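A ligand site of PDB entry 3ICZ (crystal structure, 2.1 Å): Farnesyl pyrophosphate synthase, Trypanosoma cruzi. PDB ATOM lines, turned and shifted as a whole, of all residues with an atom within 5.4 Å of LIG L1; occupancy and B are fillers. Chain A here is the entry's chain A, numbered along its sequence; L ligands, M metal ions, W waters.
Merely in contact with LIG L1: Gly 47 (3.3 Å), Arg 107 (3.95 Å), Thr 208 (3.98 Å), Tyr 211 (3.3 Å), Thr 212 (3.999 Å), Phe 246 (3.5 Å), Gln 247 (3.6 Å) and Asp 250 (3.5 Å). Hydrophobic or aromatic side chains within 4 Å of LIG L1: Phe 246. Of the 19 residues printed, 12 come within 4 Å of LIG L1. The nearest printed residue that does not touch LIG L1 is Leu 95 (4.01 Å).
NE2 of Gln 91 is in hydrogen-bond range of O5 of LIG L1. The backbone NH of Lys 48 lies within hydrogen-bond range of an oxygen (O6) of LIG L1 (2.8 Å). NZ of Lys 48 lies within salt-bridge range of O2 of LIG L1 (3.2 Å). An oxygen (O5) of LIG L1 lies within salt-bridge range of the guanidinium group (NH1) of Arg 108 (2.9 Å). NH1 of Arg 51 lies within salt-bridge range of O3 of LIG L1. An oxygen (O1) of LG2 L2 is in salt-bridge range of the guanidinium group of Arg 107. NZ of Lys 264 lies within salt-bridge range of O1 of LG2 L2.
NE2 of Gln 91 sits close to NH1 of Arg 51, 3.3 Å away. The side-chain amide oxygen (OE1) of Gln 91 lies within hydrogen-bond range of the side-chain hydroxyl (OH) of Tyr 211, 2.6 Å away. The side-chain hydroxyl (OG1) of Thr 212 is in hydrogen-bond range of the guanidinium group (NH2) of Arg 51, 3.2 Å away. The side-chain carboxylate (OD2) of Asp 250 lies close to the side-chain amide nitrogen (NE2) of Gln 247 (3.1 Å). The side-chain carboxylate (OD1) of Asp 250 lies within salt-bridge range of the side-chain amino group (NZ) of Lys 264, 2.6 Å away. The backbone carbonyl oxygen (O) of Phe 246 sits at hydrogen-bond distance from the guanidinium group (NH2) of Arg 360, at 3.0 Å. The side-chain hydroxyl of Thr 212 lies within hydrogen-bond range of the backbone carbonyl oxygen of Thr 208, at 2.9 Å.
Water W5 bridges O2 of LIG L1 (2.6 Å) and NZ of Lys 264 (3.0 Å). Water W1 lies within hydrogen-bond range of an oxygen (O6) of LIG L1 (2.7 Å), the backbone NH of Tyr 49 (3.5 Å) and the guanidinium group of Arg 51 (3.5 Å). Water W3 lies within hydrogen-bond range of O7 of LIG L1 and NH2 of Arg 107. Water W4 lies within hydrogen-bond range of the side-chain carboxylate of Glu 88, an oxygen (O5) of LIG L1, the backbone NH of Tyr 49 and the backbone NH of Lys 48. Water W2 lies within hydrogen-bond range of the guanidinium group (NH1) of Arg 360 (2.8 Å), the side-chain carboxylate (OD1) of Asp 250 (2.9 Å) and an oxygen (O2) of LIG L1 (3.1 Å).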
ATOM      1  N   GLY A  46      16.276 -30.061  -5.849  1.00  0.00           N
ATOM      2  CA  GLY A  46      16.211 -28.680  -6.293  1.00  0.00           C
ATOM      3  C   GLY A  46      15.233 -27.806  -5.592  1.00  0.00           C
ATOM      4  O   GLY A  46      15.242 -26.604  -5.825  1.00  0.00           O
ATOM      5  N   GLY A  47      14.332 -28.399  -4.801  1.00  0.00           N
ATOM      6  CA  GLY A  47      13.348 -27.604  -4.101  1.00  0.00           C
ATOM      7  C   GLY A  47      13.980 -27.054  -2.823  1.00  0.00           C
ATOM      8  O   GLY A  47      15.198 -27.205  -2.633  1.00  0.00           O
ATOM      9  N   LYS A  48      13.181 -26.464  -1.941  1.00  0.00           N
ATOM     10  CA  LYS A  48      13.730 -25.964  -0.627  1.00  0.00           C
ATOM     11  C   LYS A  48      13.868 -27.037   0.492  1.00  0.00           C
ATOM     12  O   LYS A  48      14.433 -26.761   1.534  1.00  0.00           O
ATOM     13  CB  LYS A  48      12.816 -24.854  -0.116  1.00  0.00           C
ATOM     14  CG  LYS A  48      12.863 -23.516  -0.904  1.00  0.00           C
ATOM     15  CD  LYS A  48      11.633 -22.684  -0.519  1.00  0.00           C
ATOM     16  CE  LYS A  48      10.524 -23.011  -1.515  1.00  0.00           C
ATOM     17  NZ  LYS A  48       9.323 -23.162  -0.805  1.00  0.00           N
ATOM     18  N   TYR A  49      13.350 -28.249   0.263  1.00  0.00           N
ATOM     19  CA  TYR A  49      13.301 -29.371   1.220  1.00  0.00           C
ATOM     20  C   TYR A  49      12.652 -29.006   2.542  1.00  0.00           C
ATOM     21  O   TYR A  49      13.008 -29.604   3.606  1.00  0.00           O
ATOM     22  CB  TYR A  49      14.722 -29.937   1.468  1.00  0.00           C
ATOM     23  CG  TYR A  49      15.494 -30.251   0.209  1.00  0.00           C
ATOM     24  CD1 TYR A  49      16.674 -29.559  -0.105  1.00  0.00           C
ATOM     25  CD2 TYR A  49      15.019 -31.223  -0.700  1.00  0.00           C
ATOM     26  CE1 TYR A  49      17.401 -29.826  -1.289  1.00  0.00           C
ATOM     27  CE2 TYR A  49      15.729 -31.508  -1.910  1.00  0.00           C
ATOM     28  CZ  TYR A  49      16.914 -30.788  -2.182  1.00  0.00           C
ATOM     29  OH  TYR A  49      17.624 -31.017  -3.295  1.00  0.00           O
ATOM     30  N   ARG A  51       9.519 -29.443   3.605  1.00  0.00           N
ATOM     31  CA  ARG A  51       8.631 -30.473   4.137  1.00  0.00           C
ATOM     32  C   ARG A  51       9.572 -31.557   4.730  1.00  0.00           C
ATOM     33  O   ARG A  51       9.390 -31.935   5.884  1.00  0.00           O
ATOM     34  CB  ARG A  51       7.770 -31.068   3.033  1.00  0.00           C
ATOM     35  CG  ARG A  51       6.693 -30.104   2.439  1.00  0.00           C
ATOM     36  CD  ARG A  51       6.052 -30.753   1.169  1.00  0.00           C
ATOM     37  NE  ARG A  51       5.245 -29.741   0.534  1.00  0.00           N
ATOM     38  CZ  ARG A  51       5.770 -28.683  -0.079  1.00  0.00           C
ATOM     39  NH1 ARG A  51       7.115 -28.573  -0.153  1.00  0.00           N
ATOM     40  NH2 ARG A  51       4.966 -27.748  -0.604  1.00  0.00           N
ATOM     41  N   GLU A  88       8.965 -35.678   0.251  1.00  0.00           N
ATOM     42  CA  GLU A  88       9.538 -34.996  -0.903  1.00  0.00           C
ATOM     43  C   GLU A  88       9.187 -35.707  -2.228  1.00  0.00           C
ATOM     44  O   GLU A  88       9.003 -35.067  -3.280  1.00  0.00           O
ATOM     45  CB  GLU A  88      11.016 -34.908  -0.764  1.00  0.00           C
ATOM     46  CG  GLU A  88      11.518 -33.989   0.427  1.00  0.00           C
ATOM     47  CD  GLU A  88      11.175 -32.533   0.192  1.00  0.00           C
ATOM     48  OE1 GLU A  88      11.190 -32.051  -1.001  1.00  0.00           O
ATOM     49  OE2 GLU A  88      10.866 -31.845   1.202  1.00  0.00           O
ATOM     50  N   GLN A  91       5.529 -34.885  -2.923  1.00  0.00           N
ATOM     51  CA  GLN A  91       5.644 -33.560  -3.546  1.00  0.00           C
ATOM     52  C   GLN A  91       6.084 -33.688  -5.036  1.00  0.00           C
ATOM     53  O   GLN A  91       5.445 -33.129  -5.939  1.00  0.00           O
ATOM     54  CB  GLN A  91       6.608 -32.675  -2.710  1.00  0.00           C
ATOM     55  CG  GLN A  91       7.234 -31.378  -3.444  1.00  0.00           C
ATOM     56  CD  GLN A  91       6.275 -30.190  -3.503  1.00  0.00           C
ATOM     57  OE1 GLN A  91       5.053 -30.337  -3.581  1.00  0.00           O
ATOM     58  NE2 GLN A  91       6.826 -29.005  -3.458  1.00  0.00           N
ATOM     59  N   LEU A  95       3.963 -32.341  -8.073  1.00  0.00           N
ATOM     60  CA  LEU A  95       4.505 -31.325  -8.983  1.00  0.00           C
ATOM     61  C   LEU A  95       4.496 -31.770 -10.477  1.00  0.00           C
ATOM     62  O   LEU A  95       4.158 -30.989 -11.346  1.00  0.00           O
ATOM     63  CB  LEU A  95       5.919 -30.928  -8.479  1.00  0.00           C
ATOM     64  CG  LEU A  95       6.050 -29.692  -7.603  1.00  0.00           C
ATOM     65  CD1 LEU A  95       4.800 -29.302  -6.753  1.00  0.00           C
ATOM     66  CD2 LEU A  95       7.412 -29.443  -6.939  1.00  0.00           C
ATOM     67  N   ARG A 107      10.073 -25.296 -13.714  1.00  0.00           N
ATOM     68  CA  ARG A 107       9.971 -25.803 -12.343  1.00  0.00           C
ATOM     69  C   ARG A 107      11.407 -25.927 -11.737  1.00  0.00           C
ATOM     70  O   ARG A 107      12.282 -26.556 -12.338  1.00  0.00           O
ATOM     71  CB  ARG A 107       9.356 -27.191 -12.360  1.00  0.00           C
ATOM     72  CG  ARG A 107       9.232 -27.795 -10.929  1.00  0.00           C
ATOM     73  CD  ARG A 107       7.777 -27.815 -10.676  1.00  0.00           C
ATOM     74  NE  ARG A 107       7.450 -26.934  -9.664  1.00  0.00           N
ATOM     75  CZ  ARG A 107       6.235 -26.543  -9.315  1.00  0.00           C
ATOM     76  NH1 ARG A 107       5.136 -26.927  -9.954  1.00  0.00           N
ATOM     77  NH2 ARG A 107       6.185 -25.745  -8.267  1.00  0.00           N
ATOM     78  N   ARG A 108      11.598 -25.397 -10.545  1.00  0.00           N
ATOM     79  CA  ARG A 108      12.930 -25.313  -9.887  1.00  0.00           C
ATOM     80  C   ARG A 108      14.022 -24.871 -10.877  1.00  0.00           C
ATOM     81  O   ARG A 108      15.156 -25.357 -10.840  1.00  0.00           O
ATOM     82  CB  ARG A 108      13.317 -26.556  -8.994  1.00  0.00           C
ATOM     83  CG  ARG A 108      12.073 -27.305  -8.532  1.00  0.00           C
ATOM     84  CD  ARG A 108      11.897 -27.759  -7.099  1.00  0.00           C
ATOM     85  NE  ARG A 108      12.030 -29.162  -7.111  1.00  0.00           N
ATOM     86  CZ  ARG A 108      11.383 -30.125  -6.442  1.00  0.00           C
ATOM     87  NH1 ARG A 108      10.428 -29.995  -5.543  1.00  0.00           N
ATOM     88  NH2 ARG A 108      11.793 -31.325  -6.768  1.00  0.00           N
ATOM     89  N   THR A 208      -3.228 -27.977  -0.243  1.00  0.00           N
ATOM     90  CA  THR A 208      -1.840 -27.770   0.217  1.00  0.00           C
ATOM     91  C   THR A 208      -1.492 -28.014   1.664  1.00  0.00           C
ATOM     92  O   THR A 208      -0.416 -28.508   1.941  1.00  0.00           O
ATOM     93  CB  THR A 208      -1.122 -26.468  -0.319  1.00  0.00           C
ATOM     94  OG1 THR A 208      -1.006 -25.480   0.680  1.00  0.00           O
ATOM     95  CG2 THR A 208      -1.697 -25.923  -1.569  1.00  0.00           C
ATOM     96  N   TYR A 211      -0.600 -31.772   3.145  1.00  0.00           N
ATOM     97  CA  TYR A 211       0.677 -32.457   2.745  1.00  0.00           C
ATOM     98  C   TYR A 211       1.885 -31.592   2.996  1.00  0.00           C
ATOM     99  O   TYR A 211       2.981 -32.098   3.141  1.00  0.00           O
ATOM    100  CB  TYR A 211       0.708 -32.982   1.291  1.00  0.00           C
ATOM    101  CG  TYR A 211       1.279 -32.071   0.198  1.00  0.00           C
ATOM    102  CD1 TYR A 211       2.619 -32.137  -0.161  1.00  0.00           C
ATOM    103  CD2 TYR A 211       0.467 -31.137  -0.438  1.00  0.00           C
ATOM    104  CE1 TYR A 211       3.123 -31.315  -1.184  1.00  0.00           C
ATOM    105  CE2 TYR A 211       0.947 -30.315  -1.461  1.00  0.00           C
ATOM    106  CZ  TYR A 211       2.271 -30.410  -1.827  1.00  0.00           C
ATOM    107  OH  TYR A 211       2.705 -29.616  -2.800  1.00  0.00           O
ATOM    108  N   THR A 212       1.674 -30.283   3.097  1.00  0.00           N
ATOM    109  CA  THR A 212       2.821 -29.384   3.237  1.00  0.00           C
ATOM    110  C   THR A 212       3.147 -29.129   4.725  1.00  0.00           C
ATOM    111  O   THR A 212       4.302 -28.930   5.063  1.00  0.00           O
ATOM    112  CB  THR A 212       2.590 -28.081   2.482  1.00  0.00           C
ATOM    113  OG1 THR A 212       2.378 -28.424   1.089  1.00  0.00           O
ATOM    114  CG2 THR A 212       3.796 -27.127   2.604  1.00  0.00           C
ATOM    115  N   PHE A 246       1.174 -20.015   3.565  1.00  0.00           N
ATOM    116  CA  PHE A 246       2.125 -20.556   2.584  1.00  0.00           C
ATOM    117  C   PHE A 246       1.521 -20.518   1.177  1.00  0.00           C
ATOM    118  O   PHE A 246       2.184 -20.105   0.206  1.00  0.00           O
ATOM    119  CB  PHE A 246       2.582 -21.990   2.985  1.00  0.00           C
ATOM    120  CG  PHE A 246       3.581 -22.599   2.031  1.00  0.00           C
ATOM    121  CD1 PHE A 246       3.159 -23.274   0.906  1.00  0.00           C
ATOM    122  CD2 PHE A 246       4.945 -22.418   2.215  1.00  0.00           C
ATOM    123  CE1 PHE A 246       4.037 -23.763  -0.013  1.00  0.00           C
ATOM    124  CE2 PHE A 246       5.847 -22.923   1.281  1.00  0.00           C
ATOM    125  CZ  PHE A 246       5.397 -23.601   0.180  1.00  0.00           C
ATOM    126  N   GLN A 247       0.276 -20.925   1.025  1.00  0.00           N
ATOM    127  CA  GLN A 247      -0.333 -20.882  -0.289  1.00  0.00           C
ATOM    128  C   GLN A 247      -0.592 -19.448  -0.777  1.00  0.00           C
ATOM    129  O   GLN A 247      -0.550 -19.177  -1.999  1.00  0.00           O
ATOM    130  CB  GLN A 247      -1.614 -21.693  -0.373  1.00  0.00           C
ATOM    131  CG  GLN A 247      -2.224 -21.814  -1.839  1.00  0.00           C
ATOM    132  CD  GLN A 247      -1.267 -22.511  -2.810  1.00  0.00           C
ATOM    133  OE1 GLN A 247      -0.634 -23.510  -2.452  1.00  0.00           O
ATOM    134  NE2 GLN A 247      -1.165 -21.985  -4.044  1.00  0.00           N
ATOM    135  N   ASP A 250       2.556 -18.236  -2.270  1.00  0.00           N
ATOM    136  CA  ASP A 250       2.744 -18.875  -3.550  1.00  0.00           C
ATOM    137  C   ASP A 250       1.974 -18.100  -4.606  1.00  0.00           C
ATOM    138  O   ASP A 250       2.505 -17.871  -5.680  1.00  0.00           O
ATOM    139  CB  ASP A 250       2.210 -20.302  -3.538  1.00  0.00           C
ATOM    140  CG  ASP A 250       2.512 -21.030  -4.828  1.00  0.00           C
ATOM    141  OD1 ASP A 250       3.722 -21.125  -5.206  1.00  0.00           O
ATOM    142  OD2 ASP A 250       1.539 -21.495  -5.478  1.00  0.00           O
ATOM    143  N   LYS A 264      10.055 -20.698 -11.223  1.00  0.00           N
ATOM    144  CA  LYS A 264       8.912 -21.090 -12.076  1.00  0.00           C
ATOM    145  C   LYS A 264       8.316 -19.896 -12.771  1.00  0.00           C
ATOM    146  O   LYS A 264       8.571 -18.743 -12.372  1.00  0.00           O
ATOM    147  CB  LYS A 264       7.830 -21.867 -11.283  1.00  0.00           C
ATOM    148  CG  LYS A 264       7.404 -21.288  -9.938  1.00  0.00           C
ATOM    149  CD  LYS A 264       6.515 -22.306  -9.128  1.00  0.00           C
ATOM    150  CE  LYS A 264       5.923 -21.647  -7.888  1.00  0.00           C
ATOM    151  NZ  LYS A 264       5.186 -22.532  -6.874  1.00  0.00           N
ATOM    152  N   ARG A 360      10.575 -16.632   3.589  1.00  0.00           N
ATOM    153  CA  ARG A 360      10.867 -17.133   2.232  1.00  0.00           C
ATOM    154  C   ARG A 360      10.521 -16.121   1.120  1.00  0.00           C
ATOM    155  O   ARG A 360       9.561 -15.350   1.201  1.00  0.00           O
ATOM    156  CB  ARG A 360      10.210 -18.495   1.942  1.00  0.00           C
ATOM    157  CG  ARG A 360       8.834 -18.414   1.290  1.00  0.00           C
ATOM    158  CD  ARG A 360       7.978 -19.703   1.601  1.00  0.00           C
ATOM    159  NE  ARG A 360       6.650 -19.713   1.015  1.00  0.00           N
ATOM    160  CZ  ARG A 360       6.359 -20.101  -0.244  1.00  0.00           C
ATOM    161  NH1 ARG A 360       7.290 -20.527  -1.072  1.00  0.00           N
ATOM    162  NH2 ARG A 360       5.111 -20.171  -0.641  1.00  0.00           N
ATOM    163  N   LYS A 362      10.995 -17.336  -2.054  1.00  0.00           N
ATOM    164  CA  LYS A 362      10.647 -18.339  -3.016  1.00  0.00           C
ATOM    165  C   LYS A 362      10.209 -19.615  -2.326  1.00  0.00           C
ATOM    166  O   LYS A 362       9.938 -20.541  -3.095  1.00  0.00           O
ATOM    167  CB  LYS A 362      11.804 -18.645  -3.936  1.00  0.00           C
ATOM    168  CG  LYS A 362      13.011 -19.181  -3.180  1.00  0.00           C
ATOM    169  CD  LYS A 362      14.131 -19.543  -4.145  1.00  0.00           C
ATOM    170  CE  LYS A 362      14.086 -20.984  -4.543  1.00  0.00           C
ATOM    171  NZ  LYS A 362      15.210 -21.321  -5.483  1.00  0.00           N
HETATM  172  C1  LIG L   1       5.261 -25.774  -4.425  1.00  0.00           C
HETATM  173  O1  LIG L   1       5.798 -26.042  -3.137  1.00  0.00           O
HETATM  174  C2  LIG L   1       3.787 -26.200  -4.424  1.00  0.00           C
HETATM  175  C3  LIG L   1       2.964 -25.471  -3.369  1.00  0.00           C
HETATM  176  C4  LIG L   1       2.810 -24.141  -3.317  1.00  0.00           C
HETATM  177  C5  LIG L   1       2.308 -26.354  -2.332  1.00  0.00           C
HETATM  178  P1  LIG L   1       7.288 -25.494  -2.777  1.00  0.00           P
HETATM  179  O2  LIG L   1       7.313 -24.058  -3.130  1.00  0.00           O
HETATM  180  O3  LIG L   1       7.655 -25.996  -1.393  1.00  0.00           O
HETATM  181  O4  LIG L   1       8.257 -26.268  -3.842  1.00  0.00           O
HETATM  182  P2  LIG L   1       9.752 -26.883  -3.622  1.00  0.00           P
HETATM  183  O5  LIG L   1       9.560 -28.376  -3.337  1.00  0.00           O
HETATM  184  O6  LIG L   1      10.436 -26.123  -2.583  1.00  0.00           O
HETATM  185  O7  LIG L   1      10.323 -26.543  -4.973  1.00  0.00           O
HETATM  186  C1  LG2 L   2       1.596 -26.598  -7.076  1.00  0.00           C
HETATM  187  C2  LG2 L   2       1.441 -25.059  -7.013  1.00  0.00           C
HETATM  188  P1  LG2 L   2       2.756 -24.403  -8.085  1.00  0.00           P
HETATM  189  O1  LG2 L   2       4.063 -24.868  -7.530  1.00  0.00           O
HETATM  190  O2  LG2 L   2       2.669 -22.883  -7.995  1.00  0.00           O
HETATM  191  N1  LG2 L   2       0.689 -27.348  -6.135  1.00  0.00           N
HETATM  192  O3  LG2 L   2       2.427 -24.896  -9.434  1.00  0.00           O
HETATM  193  C3  LG2 L   2       0.238 -26.886  -4.913  1.00  0.00           C
HETATM  194  C4  LG2 L   2      -0.644 -27.693  -4.173  1.00  0.00           C
HETATM  195  P2  LG2 L   2      -0.229 -24.509  -7.551  1.00  0.00           P
HETATM  196  C5  LG2 L   2      -1.046 -28.971  -4.660  1.00  0.00           C
HETATM  197  O4  LG2 L   2      -0.474 -25.231  -8.850  1.00  0.00           O
HETATM  198  C6  LG2 L   2      -0.550 -29.403  -5.915  1.00  0.00           C
HETATM  199  O5  LG2 L   2      -1.268 -25.036  -6.607  1.00  0.00           O
HETATM  200  C7  LG2 L   2       0.283 -28.529  -6.594  1.00  0.00           C
HETATM  201  O6  LG2 L   2      -0.201 -22.979  -7.486  1.00  0.00           O
HETATM  202  C8  LG2 L   2      -0.886 -30.673  -6.653  1.00  0.00           C
HETATM  203  C9  LG2 L   2      -1.698 -31.578  -6.139  1.00  0.00           C
HETATM  204  C10 LG2 L   2      -2.101 -32.905  -6.776  1.00  0.00           C
HETATM  205  C11 LG2 L   2      -1.524 -33.119  -8.155  1.00  0.00           C
HETATM  206 MG    MG M   1       1.304 -21.571  -7.462  1.00  0.00          MG
HETATM  207  O   HOH W   1      10.160 -26.939   0.026  1.00  0.00           O
HETATM  208  O   HOH W   2       5.679 -21.405  -3.130  1.00  0.00           O
HETATM  209  O   HOH W   3       8.745 -25.356  -6.918  1.00  0.00           O
HETATM  210  O   HOH W   4      11.659 -29.522  -1.926  1.00  0.00           O
HETATM  211  O   HOH W   5       7.718 -23.319  -5.564  1.00  0.00           O
HETATM  212  O   HOH W   6      11.694 -24.163  -4.794  1.00  0.00           O
